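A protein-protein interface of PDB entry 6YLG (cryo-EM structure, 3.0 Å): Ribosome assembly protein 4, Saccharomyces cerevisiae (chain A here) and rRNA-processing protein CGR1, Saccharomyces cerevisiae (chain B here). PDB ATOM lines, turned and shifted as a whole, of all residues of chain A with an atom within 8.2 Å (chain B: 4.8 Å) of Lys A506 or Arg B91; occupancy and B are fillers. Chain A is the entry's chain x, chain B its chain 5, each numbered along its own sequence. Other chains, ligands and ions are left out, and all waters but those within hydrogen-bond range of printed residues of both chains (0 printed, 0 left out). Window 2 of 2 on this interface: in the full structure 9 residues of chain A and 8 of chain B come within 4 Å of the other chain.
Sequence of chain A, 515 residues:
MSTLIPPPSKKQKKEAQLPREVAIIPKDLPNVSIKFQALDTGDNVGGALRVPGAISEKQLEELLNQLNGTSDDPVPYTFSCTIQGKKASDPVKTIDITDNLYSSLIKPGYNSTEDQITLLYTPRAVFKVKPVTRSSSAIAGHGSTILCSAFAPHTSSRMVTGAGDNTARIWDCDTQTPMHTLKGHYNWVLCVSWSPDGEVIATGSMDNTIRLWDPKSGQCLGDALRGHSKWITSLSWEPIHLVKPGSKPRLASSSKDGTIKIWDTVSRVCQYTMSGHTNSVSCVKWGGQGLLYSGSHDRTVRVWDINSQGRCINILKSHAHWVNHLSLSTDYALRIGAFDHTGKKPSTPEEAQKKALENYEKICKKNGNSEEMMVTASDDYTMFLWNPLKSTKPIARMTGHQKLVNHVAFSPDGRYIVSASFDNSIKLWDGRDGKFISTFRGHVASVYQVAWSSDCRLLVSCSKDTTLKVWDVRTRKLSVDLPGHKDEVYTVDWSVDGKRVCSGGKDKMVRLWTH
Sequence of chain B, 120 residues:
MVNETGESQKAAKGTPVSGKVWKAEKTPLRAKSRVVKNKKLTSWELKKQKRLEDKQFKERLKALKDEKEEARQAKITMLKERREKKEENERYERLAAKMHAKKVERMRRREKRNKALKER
The side-chain carboxylate (OD2) of Asp A487 is in salt-bridge range of the guanidinium group (NH2) of Arg B91, 3.5 Å away. The side-chain carboxylate (OE2) of Glu B88 lies within salt-bridge range of the side-chain amino group (NZ) of Lys A508, at 3.8 Å.
Lys A506 touches one residue of chain B. Arg B91 touches two residues of chain A. Of the printed residues of chain B, Asp A487 touches Arg B91, Tyr B92 and Leu B95. Printed residues of chain A within 4 Å of Leu B95: Asp A487. Met A509 touches none of the printed residues of chain B. Ser A503 touches none of the printed residues of chain B. The nearest residue of chain A that does not touch Arg B91 is Lys A508 (5.2 Å).
Of the 22 printed residues of chain A, 5 touch a printed residue of chain B. Hydrophobic or aromatic side chains of chain B that line the printed part of chain A: Tyr B92 and Leu B95. Along chain B the printed residues that touch a printed residue of chain A span positions 88 to 95.
Among the printed residues, pairs that only touch across the chains: Asp A487 with Leu B95 (3.3 Å), Asp A487 with Tyr B92 (3.6 Å), Lys A486 with Tyr B92 (3.7 Å), Lys A506 with Arg B91 (3.7 Å) and Asp A507 with Tyr B92 (3.8 Å).
The backbone carbonyl oxygen (O) of Glu A488 lies within hydrogen-bond range of the backbone NH (N) of Lys A506 (2.9 Å). NZ of Lys A506 is in hydrogen-bond range of OH of Tyr A490, 2.6 Å away. OD1 of Asp A507 lies within hydrogen-bond range of ND1 of His A485 (3.2 Å). The side-chain hydroxyl (OH) of Tyr B92 lies within hydrogen-bond range of the side-chain carboxylate (OE2) of Glu B88 (2.5 Å).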
ATOM      1  N   GLY A 143       7.850  10.720  10.396  1.00  0.00           N
ATOM      2  CA  GLY A 143       7.344   9.391  10.665  1.00  0.00           C
ATOM      3  C   GLY A 143       6.690   9.218  12.019  1.00  0.00           C
ATOM      4  O   GLY A 143       7.162   8.438  12.851  1.00  0.00           O
ATOM      5  N   SER A 144       5.606   9.945  12.251  1.00  0.00           N
ATOM      6  CA  SER A 144       4.714   9.578  13.342  1.00  0.00           C
ATOM      7  C   SER A 144       3.340  10.153  13.015  1.00  0.00           C
ATOM      8  O   SER A 144       3.117  10.680  11.919  1.00  0.00           O
ATOM      9  CB  SER A 144       5.269  10.062  14.686  1.00  0.00           C
ATOM     10  OG  SER A 144       5.662  11.420  14.625  1.00  0.00           O
ATOM     11  N   THR A 145       2.429  10.144  13.983  1.00  0.00           N
ATOM     12  CA  THR A 145       1.028  10.435  13.707  1.00  0.00           C
ATOM     13  C   THR A 145       0.865  11.860  13.193  1.00  0.00           C
ATOM     14  O   THR A 145       1.369  12.812  13.797  1.00  0.00           O
ATOM     15  CB  THR A 145       0.195  10.229  14.971  1.00  0.00           C
ATOM     16  OG1 THR A 145       0.132   8.832  15.282  1.00  0.00           O
ATOM     17  CG2 THR A 145      -1.218  10.758  14.792  1.00  0.00           C
ATOM     18  N   ILE A 146       0.158  12.003  12.071  1.00  0.00           N
ATOM     19  CA  ILE A 146      -0.163  13.326  11.553  1.00  0.00           C
ATOM     20  C   ILE A 146      -1.303  13.907  12.375  1.00  0.00           C
ATOM     21  O   ILE A 146      -2.259  13.200  12.720  1.00  0.00           O
ATOM     22  CB  ILE A 146      -0.527  13.257  10.064  1.00  0.00           C
ATOM     23  CG1 ILE A 146       0.693  12.854   9.233  1.00  0.00           C
ATOM     24  CG2 ILE A 146      -1.057  14.603   9.589  1.00  0.00           C
ATOM     25  CD1 ILE A 146       0.362  12.344   7.847  1.00  0.00           C
ATOM     26  N   LEU A 147      -1.207  15.198  12.693  1.00  0.00           N
ATOM     27  CA  LEU A 147      -2.144  15.856  13.592  1.00  0.00           C
ATOM     28  C   LEU A 147      -2.770  17.110  13.005  1.00  0.00           C
ATOM     29  O   LEU A 147      -3.942  17.388  13.282  1.00  0.00           O
ATOM     30  CB  LEU A 147      -1.441  16.194  14.912  1.00  0.00           C
ATOM     31  CG  LEU A 147      -1.088  14.980  15.775  1.00  0.00           C
ATOM     32  CD1 LEU A 147      -0.170  15.379  16.913  1.00  0.00           C
ATOM     33  CD2 LEU A 147      -2.339  14.294  16.304  1.00  0.00           C
ATOM     34  N   TYR A 448     -14.556  13.676  12.541  1.00  0.00           N
ATOM     35  CA  TYR A 448     -13.684  14.619  13.231  1.00  0.00           C
ATOM     36  C   TYR A 448     -13.819  16.029  12.670  1.00  0.00           C
ATOM     37  O   TYR A 448     -14.027  16.976  13.432  1.00  0.00           O
ATOM     38  CB  TYR A 448     -12.230  14.133  13.156  1.00  0.00           C
ATOM     39  CG  TYR A 448     -11.966  12.789  13.822  1.00  0.00           C
ATOM     40  CD1 TYR A 448     -12.681  12.380  14.943  1.00  0.00           C
ATOM     41  CD2 TYR A 448     -10.993  11.934  13.330  1.00  0.00           C
ATOM     42  CE1 TYR A 448     -12.437  11.164  15.541  1.00  0.00           C
ATOM     43  CE2 TYR A 448     -10.743  10.715  13.924  1.00  0.00           C
ATOM     44  CZ  TYR A 448     -11.467  10.336  15.029  1.00  0.00           C
ATOM     45  OH  TYR A 448     -11.222   9.122  15.626  1.00  0.00           O
ATOM     46  N   LYS A 464     -13.281   8.723  11.663  1.00  0.00           N
ATOM     47  CA  LYS A 464     -12.513   7.702  12.362  1.00  0.00           C
ATOM     48  C   LYS A 464     -12.317   6.477  11.487  1.00  0.00           C
ATOM     49  O   LYS A 464     -11.314   5.769  11.626  1.00  0.00           O
ATOM     50  CB  LYS A 464     -13.221   7.335  13.663  1.00  0.00           C
ATOM     51  CG  LYS A 464     -12.573   6.221  14.460  1.00  0.00           C
ATOM     52  CD  LYS A 464     -13.163   6.152  15.856  1.00  0.00           C
ATOM     53  CE  LYS A 464     -12.396   5.198  16.743  1.00  0.00           C
ATOM     54  NZ  LYS A 464     -12.871   5.273  18.147  1.00  0.00           N
ATOM     55  N   THR A 466     -11.359   4.974   7.770  1.00  0.00           N
ATOM     56  CA  THR A 466     -10.216   5.372   6.959  1.00  0.00           C
ATOM     57  C   THR A 466     -10.603   6.169   5.722  1.00  0.00           C
ATOM     58  O   THR A 466      -9.721   6.473   4.915  1.00  0.00           O
ATOM     59  CB  THR A 466      -9.424   4.136   6.534  1.00  0.00           C
ATOM     60  OG1 THR A 466     -10.160   3.414   5.540  1.00  0.00           O
ATOM     61  CG2 THR A 466      -9.166   3.232   7.730  1.00  0.00           C
ATOM     62  N   HIS A 485      -6.556   5.541   2.734  1.00  0.00           N
ATOM     63  CA  HIS A 485      -5.854   5.492   4.005  1.00  0.00           C
ATOM     64  C   HIS A 485      -6.055   4.118   4.639  1.00  0.00           C
ATOM     65  O   HIS A 485      -6.816   3.281   4.143  1.00  0.00           O
ATOM     66  CB  HIS A 485      -6.347   6.592   4.945  1.00  0.00           C
ATOM     67  CG  HIS A 485      -5.824   7.957   4.618  1.00  0.00           C
ATOM     68  ND1 HIS A 485      -4.643   8.445   5.133  1.00  0.00           N
ATOM     69  CD2 HIS A 485      -6.336   8.945   3.848  1.00  0.00           C
ATOM     70  CE1 HIS A 485      -4.442   9.670   4.683  1.00  0.00           C
ATOM     71  NE2 HIS A 485      -5.454   9.998   3.900  1.00  0.00           N
ATOM     72  N   LYS A 486      -5.357   3.888   5.752  1.00  0.00           N
ATOM     73  CA  LYS A 486      -5.384   2.608   6.452  1.00  0.00           C
ATOM     74  C   LYS A 486      -5.648   2.758   7.943  1.00  0.00           C
ATOM     75  O   LYS A 486      -5.492   1.783   8.688  1.00  0.00           O
ATOM     76  CB  LYS A 486      -4.063   1.864   6.234  1.00  0.00           C
ATOM     77  CG  LYS A 486      -3.768   1.521   4.773  1.00  0.00           C
ATOM     78  CD  LYS A 486      -2.285   1.275   4.501  1.00  0.00           C
ATOM     79  CE  LYS A 486      -1.896   1.797   3.128  1.00  0.00           C
ATOM     80  NZ  LYS A 486      -0.455   1.598   2.831  1.00  0.00           N
ATOM     81  N   ASP A 487      -6.044   3.940   8.404  1.00  0.00           N
ATOM     82  CA  ASP A 487      -6.288   4.172   9.822  1.00  0.00           C
ATOM     83  C   ASP A 487      -7.086   5.463   9.965  1.00  0.00           C
ATOM     84  O   ASP A 487      -7.577   6.023   8.979  1.00  0.00           O
ATOM     85  CB  ASP A 487      -4.972   4.221  10.605  1.00  0.00           C
ATOM     86  CG  ASP A 487      -5.101   3.632  11.991  1.00  0.00           C
ATOM     87  OD1 ASP A 487      -6.156   3.834  12.624  1.00  0.00           O
ATOM     88  OD2 ASP A 487      -4.148   2.967  12.446  1.00  0.00           O
ATOM     89  N   GLU A 488      -7.220   5.931  11.202  1.00  0.00           N
ATOM     90  CA  GLU A 488      -8.029   7.107  11.486  1.00  0.00           C
ATOM     91  C   GLU A 488      -7.436   8.346  10.828  1.00  0.00           C
ATOM     92  O   GLU A 488      -6.241   8.625  10.955  1.00  0.00           O
ATOM     93  CB  GLU A 488      -8.138   7.321  12.995  1.00  0.00           C
ATOM     94  CG  GLU A 488      -8.680   6.126  13.762  1.00  0.00           C
ATOM     95  CD  GLU A 488      -8.819   6.400  15.245  1.00  0.00           C
ATOM     96  OE1 GLU A 488      -8.705   7.575  15.647  1.00  0.00           O
ATOM     97  OE2 GLU A 488      -9.038   5.436  16.009  1.00  0.00           O
ATOM     98  N   VAL A 489      -8.286   9.090  10.127  1.00  0.00           N
ATOM     99  CA  VAL A 489      -7.897  10.316   9.439  1.00  0.00           C
ATOM    100  C   VAL A 489      -8.267  11.494  10.326  1.00  0.00           C
ATOM    101  O   VAL A 489      -9.450  11.731  10.590  1.00  0.00           O
ATOM    102  CB  VAL A 489      -8.582  10.424   8.067  1.00  0.00           C
ATOM    103  CG1 VAL A 489      -8.210  11.729   7.387  1.00  0.00           C
ATOM    104  CG2 VAL A 489      -8.209   9.238   7.194  1.00  0.00           C
ATOM    105  N   TYR A 490      -7.257  12.241  10.770  1.00  0.00           N
ATOM    106  CA  TYR A 490      -7.456  13.319  11.728  1.00  0.00           C
ATOM    107  C   TYR A 490      -7.621  14.687  11.086  1.00  0.00           C
ATOM    108  O   TYR A 490      -8.410  15.492  11.591  1.00  0.00           O
ATOM    109  CB  TYR A 490      -6.279  13.379  12.711  1.00  0.00           C
ATOM    110  CG  TYR A 490      -6.179  12.214  13.680  1.00  0.00           C
ATOM    111  CD1 TYR A 490      -7.293  11.739  14.360  1.00  0.00           C
ATOM    112  CD2 TYR A 490      -4.960  11.600  13.927  1.00  0.00           C
ATOM    113  CE1 TYR A 490      -7.197  10.686  15.239  1.00  0.00           C
ATOM    114  CE2 TYR A 490      -4.857  10.545  14.809  1.00  0.00           C
ATOM    115  CZ  TYR A 490      -5.979  10.093  15.463  1.00  0.00           C
ATOM    116  OH  TYR A 490      -5.887   9.044  16.344  1.00  0.00           O
ATOM    117  N   THR A 491      -6.907  14.974   9.996  1.00  0.00           N
ATOM    118  CA  THR A 491      -6.953  16.287   9.365  1.00  0.00           C
ATOM    119  C   THR A 491      -7.219  16.167   7.873  1.00  0.00           C
ATOM    120  O   THR A 491      -6.772  15.224   7.211  1.00  0.00           O
ATOM    121  CB  THR A 491      -5.653  17.066   9.568  1.00  0.00           C
ATOM    122  OG1 THR A 491      -5.102  16.766  10.855  1.00  0.00           O
ATOM    123  CG2 THR A 491      -5.923  18.560   9.467  1.00  0.00           C
ATOM    124  N   SER A 503      -4.936  15.301   3.108  1.00  0.00           N
ATOM    125  CA  SER A 503      -5.531  14.502   4.177  1.00  0.00           C
ATOM    126  C   SER A 503      -4.425  13.738   4.883  1.00  0.00           C
ATOM    127  O   SER A 503      -3.498  13.244   4.230  1.00  0.00           O
ATOM    128  CB  SER A 503      -6.581  13.546   3.625  1.00  0.00           C
ATOM    129  OG  SER A 503      -6.044  12.753   2.584  1.00  0.00           O
ATOM    130  N   GLY A 504      -4.517  13.640   6.201  1.00  0.00           N
ATOM    131  CA  GLY A 504      -3.501  12.957   6.979  1.00  0.00           C
ATOM    132  C   GLY A 504      -4.040  12.499   8.316  1.00  0.00           C
ATOM    133  O   GLY A 504      -4.962  13.097   8.879  1.00  0.00           O
ATOM    134  N   GLY A 505      -3.444  11.423   8.826  1.00  0.00           N
ATOM    135  CA  GLY A 505      -3.847  10.873  10.102  1.00  0.00           C
ATOM    136  C   GLY A 505      -2.836   9.938  10.733  1.00  0.00           C
ATOM    137  O   GLY A 505      -1.626  10.178  10.675  1.00  0.00           O
ATOM    138  N   LYS A 506      -3.332   8.858  11.342  1.00  0.00           N
ATOM    139  CA  LYS A 506      -2.490   7.979  12.143  1.00  0.00           C
ATOM    140  C   LYS A 506      -1.518   7.152  11.312  1.00  0.00           C
ATOM    141  O   LYS A 506      -0.492   6.717  11.843  1.00  0.00           O
ATOM    142  CB  LYS A 506      -3.364   7.048  12.980  1.00  0.00           C
ATOM    143  CG  LYS A 506      -2.611   6.300  14.072  1.00  0.00           C
ATOM    144  CD  LYS A 506      -3.534   5.404  14.898  1.00  0.00           C
ATOM    145  CE  LYS A 506      -4.544   6.181  15.732  1.00  0.00           C
ATOM    146  NZ  LYS A 506      -3.926   7.272  16.533  1.00  0.00           N
ATOM    147  N   ASP A 507      -1.807   6.919  10.034  1.00  0.00           N
ATOM    148  CA  ASP A 507      -0.968   6.064   9.204  1.00  0.00           C
ATOM    149  C   ASP A 507       0.323   6.741   8.746  1.00  0.00           C
ATOM    150  O   ASP A 507       1.058   6.156   7.944  1.00  0.00           O
ATOM    151  CB  ASP A 507      -1.757   5.572   7.986  1.00  0.00           C
ATOM    152  CG  ASP A 507      -2.199   6.702   7.075  1.00  0.00           C
ATOM    153  OD1 ASP A 507      -2.710   7.719   7.590  1.00  0.00           O
ATOM    154  OD2 ASP A 507      -2.038   6.570   5.844  1.00  0.00           O
ATOM    155  N   LYS A 508       0.605   7.960   9.215  1.00  0.00           N
ATOM    156  CA  LYS A 508       1.888   8.631   9.007  1.00  0.00           C
ATOM    157  C   LYS A 508       2.158   9.016   7.557  1.00  0.00           C
ATOM    158  O   LYS A 508       3.244   9.520   7.253  1.00  0.00           O
ATOM    159  CB  LYS A 508       3.049   7.758   9.493  1.00  0.00           C
ATOM    160  CG  LYS A 508       2.887   7.176  10.879  1.00  0.00           C
ATOM    161  CD  LYS A 508       4.105   6.354  11.246  1.00  0.00           C
ATOM    162  CE  LYS A 508       3.988   5.767  12.635  1.00  0.00           C
ATOM    163  NZ  LYS A 508       2.828   4.845  12.753  1.00  0.00           N
ATOM    164  N   MET A 509       1.197   8.794   6.661  1.00  0.00           N
ATOM    165  CA  MET A 509       1.382   8.996   5.231  1.00  0.00           C
ATOM    166  C   MET A 509       0.326   9.978   4.749  1.00  0.00           C
ATOM    167  O   MET A 509      -0.866   9.655   4.733  1.00  0.00           O
ATOM    168  CB  MET A 509       1.286   7.670   4.475  1.00  0.00           C
ATOM    169  CG  MET A 509       2.336   6.639   4.887  1.00  0.00           C
ATOM    170  SD  MET A 509       3.987   7.008   4.264  1.00  0.00           S
ATOM    171  CE  MET A 509       5.017   6.397   5.601  1.00  0.00           C
ATOM    172  N   GLU B  87       2.544  -5.244  15.010  1.00  0.00           N
ATOM    173  CA  GLU B  87       1.275  -4.807  15.580  1.00  0.00           C
ATOM    174  C   GLU B  87       0.609  -3.750  14.708  1.00  0.00           C
ATOM    175  O   GLU B  87      -0.620  -3.641  14.696  1.00  0.00           O
ATOM    176  CB  GLU B  87       1.483  -4.286  17.001  1.00  0.00           C
ATOM    177  CG  GLU B  87       2.009  -2.865  17.082  1.00  0.00           C
ATOM    178  CD  GLU B  87       2.682  -2.563  18.408  1.00  0.00           C
ATOM    179  OE1 GLU B  87       3.507  -3.382  18.863  1.00  0.00           O
ATOM    180  OE2 GLU B  87       2.380  -1.505  18.998  1.00  0.00           O
ATOM    181  N   GLU B  88       1.392  -2.984  13.941  1.00  0.00           N
ATOM    182  CA  GLU B  88       0.804  -1.993  13.048  1.00  0.00           C
ATOM    183  C   GLU B  88      -0.014  -2.661  11.954  1.00  0.00           C
ATOM    184  O   GLU B  88      -1.181  -2.305  11.733  1.00  0.00           O
ATOM    185  CB  GLU B  88       1.902  -1.122  12.436  1.00  0.00           C
ATOM    186  CG  GLU B  88       1.395  -0.010  11.532  1.00  0.00           C
ATOM    187  CD  GLU B  88       2.491   0.956  11.125  1.00  0.00           C
ATOM    188  OE1 GLU B  88       3.656   0.736  11.515  1.00  0.00           O
ATOM    189  OE2 GLU B  88       2.189   1.936  10.411  1.00  0.00           O
ATOM    190  N   ASN B  89       0.579  -3.626  11.243  1.00  0.00           N
ATOM    191  CA  ASN B  89      -0.209  -4.275  10.198  1.00  0.00           C
ATOM    192  C   ASN B  89      -1.357  -5.096  10.782  1.00  0.00           C
ATOM    193  O   ASN B  89      -2.435  -5.158  10.171  1.00  0.00           O
ATOM    194  CB  ASN B  89       0.675  -5.143   9.298  1.00  0.00           C
ATOM    195  CG  ASN B  89       1.240  -6.344  10.009  1.00  0.00           C
ATOM    196  OD1 ASN B  89       2.333  -6.285  10.562  1.00  0.00           O
ATOM    197  ND2 ASN B  89       0.512  -7.455   9.975  1.00  0.00           N
ATOM    198  N   GLU B  90      -1.166  -5.687  11.968  1.00  0.00           N
ATOM    199  CA  GLU B  90      -2.270  -6.373  12.636  1.00  0.00           C
ATOM    200  C   GLU B  90      -3.422  -5.414  12.917  1.00  0.00           C
ATOM    201  O   GLU B  90      -4.595  -5.746  12.692  1.00  0.00           O
ATOM    202  CB  GLU B  90      -1.775  -7.001  13.937  1.00  0.00           C
ATOM    203  CG  GLU B  90      -0.946  -8.251  13.740  1.00  0.00           C
ATOM    204  CD  GLU B  90       0.020  -8.489  14.880  1.00  0.00           C
ATOM    205  OE1 GLU B  90      -0.439  -8.591  16.038  1.00  0.00           O
ATOM    206  OE2 GLU B  90       1.239  -8.573  14.622  1.00  0.00           O
ATOM    207  N   ARG B  91      -3.101  -4.222  13.421  1.00  0.00           N
ATOM    208  CA  ARG B  91      -4.120  -3.231  13.736  1.00  0.00           C
ATOM    209  C   ARG B  91      -4.851  -2.778  12.484  1.00  0.00           C
ATOM    210  O   ARG B  91      -6.071  -2.594  12.505  1.00  0.00           O
ATOM    211  CB  ARG B  91      -3.469  -2.040  14.431  1.00  0.00           C
ATOM    212  CG  ARG B  91      -4.422  -1.177  15.224  1.00  0.00           C
ATOM    213  CD  ARG B  91      -3.651  -0.156  16.031  1.00  0.00           C
ATOM    214  NE  ARG B  91      -3.013   0.827  15.156  1.00  0.00           N
ATOM    215  CZ  ARG B  91      -1.885   1.485  15.421  1.00  0.00           C
ATOM    216  NH1 ARG B  91      -1.216   1.297  16.554  1.00  0.00           N
ATOM    217  NH2 ARG B  91      -1.416   2.349  14.532  1.00  0.00           N
ATOM    218  N   TYR B  92      -4.118  -2.577  11.388  1.00  0.00           N
ATOM    219  CA  TYR B  92      -4.763  -2.225  10.126  1.00  0.00           C
ATOM    220  C   TYR B  92      -5.752  -3.291   9.681  1.00  0.00           C
ATOM    221  O   TYR B  92      -6.883  -2.957   9.286  1.00  0.00           O
ATOM    222  CB  TYR B  92      -3.728  -2.029   9.012  1.00  0.00           C
ATOM    223  CG  TYR B  92      -2.774  -0.854   9.152  1.00  0.00           C
ATOM    224  CD1 TYR B  92      -2.762  -0.042  10.283  1.00  0.00           C
ATOM    225  CD2 TYR B  92      -1.877  -0.561   8.135  1.00  0.00           C
ATOM    226  CE1 TYR B  92      -1.884   1.016  10.392  1.00  0.00           C
ATOM    227  CE2 TYR B  92      -0.999   0.497   8.237  1.00  0.00           C
ATOM    228  CZ  TYR B  92      -1.006   1.281   9.367  1.00  0.00           C
ATOM    229  OH  TYR B  92      -0.133   2.336   9.470  1.00  0.00           O
ATOM    230  N   GLU B  93      -5.351  -4.562   9.757  1.00  0.00           N
ATOM    231  CA  GLU B  93      -6.248  -5.649   9.376  1.00  0.00           C
ATOM    232  C   GLU B  93      -7.498  -5.664  10.249  1.00  0.00           C
ATOM    233  O   GLU B  93      -8.624  -5.744   9.736  1.00  0.00           O
ATOM    234  CB  GLU B  93      -5.513  -6.986   9.477  1.00  0.00           C
ATOM    235  CG  GLU B  93      -5.917  -8.005   8.431  1.00  0.00           C
ATOM    236  CD  GLU B  93      -4.962  -9.182   8.375  1.00  0.00           C
ATOM    237  OE1 GLU B  93      -4.153  -9.335   9.313  1.00  0.00           O
ATOM    238  OE2 GLU B  93      -5.017  -9.950   7.393  1.00  0.00           O
ATOM    239  N   ARG B  94      -7.316  -5.585  11.571  1.00  0.00           N
ATOM    240  CA  ARG B  94      -8.460  -5.619  12.475  1.00  0.00           C
ATOM    241  C   ARG B  94      -9.376  -4.421  12.269  1.00  0.00           C
ATOM    242  O   ARG B  94     -10.599  -4.552  12.371  1.00  0.00           O
ATOM    243  CB  ARG B  94      -7.983  -5.673  13.924  1.00  0.00           C
ATOM    244  CG  ARG B  94      -7.309  -6.977  14.300  1.00  0.00           C
ATOM    245  CD  ARG B  94      -7.339  -7.197  15.800  1.00  0.00           C
ATOM    246  NE  ARG B  94      -6.954  -5.995  16.539  1.00  0.00           N
ATOM    247  CZ  ARG B  94      -5.702  -5.626  16.807  1.00  0.00           C
ATOM    248  NH1 ARG B  94      -5.483  -4.512  17.490  1.00  0.00           N
ATOM    249  NH2 ARG B  94      -4.664  -6.348  16.398  1.00  0.00           N
ATOM    250  N   LEU B  95      -8.810  -3.255  11.962  1.00  0.00           N
ATOM    251  CA  LEU B  95      -9.631  -2.067  11.760  1.00  0.00           C
ATOM    252  C   LEU B  95     -10.466  -2.182  10.492  1.00  0.00           C
ATOM    253  O   LEU B  95     -11.655  -1.829  10.488  1.00  0.00           O
ATOM    254  CB  LEU B  95      -8.737  -0.831  11.706  1.00  0.00           C
ATOM    255  CG  LEU B  95      -9.396   0.527  11.942  1.00  0.00           C
ATOM    256  CD1 LEU B  95      -9.958   0.637  13.351  1.00  0.00           C
ATOM    257  CD2 LEU B  95      -8.386   1.620  11.679  1.00  0.00           C
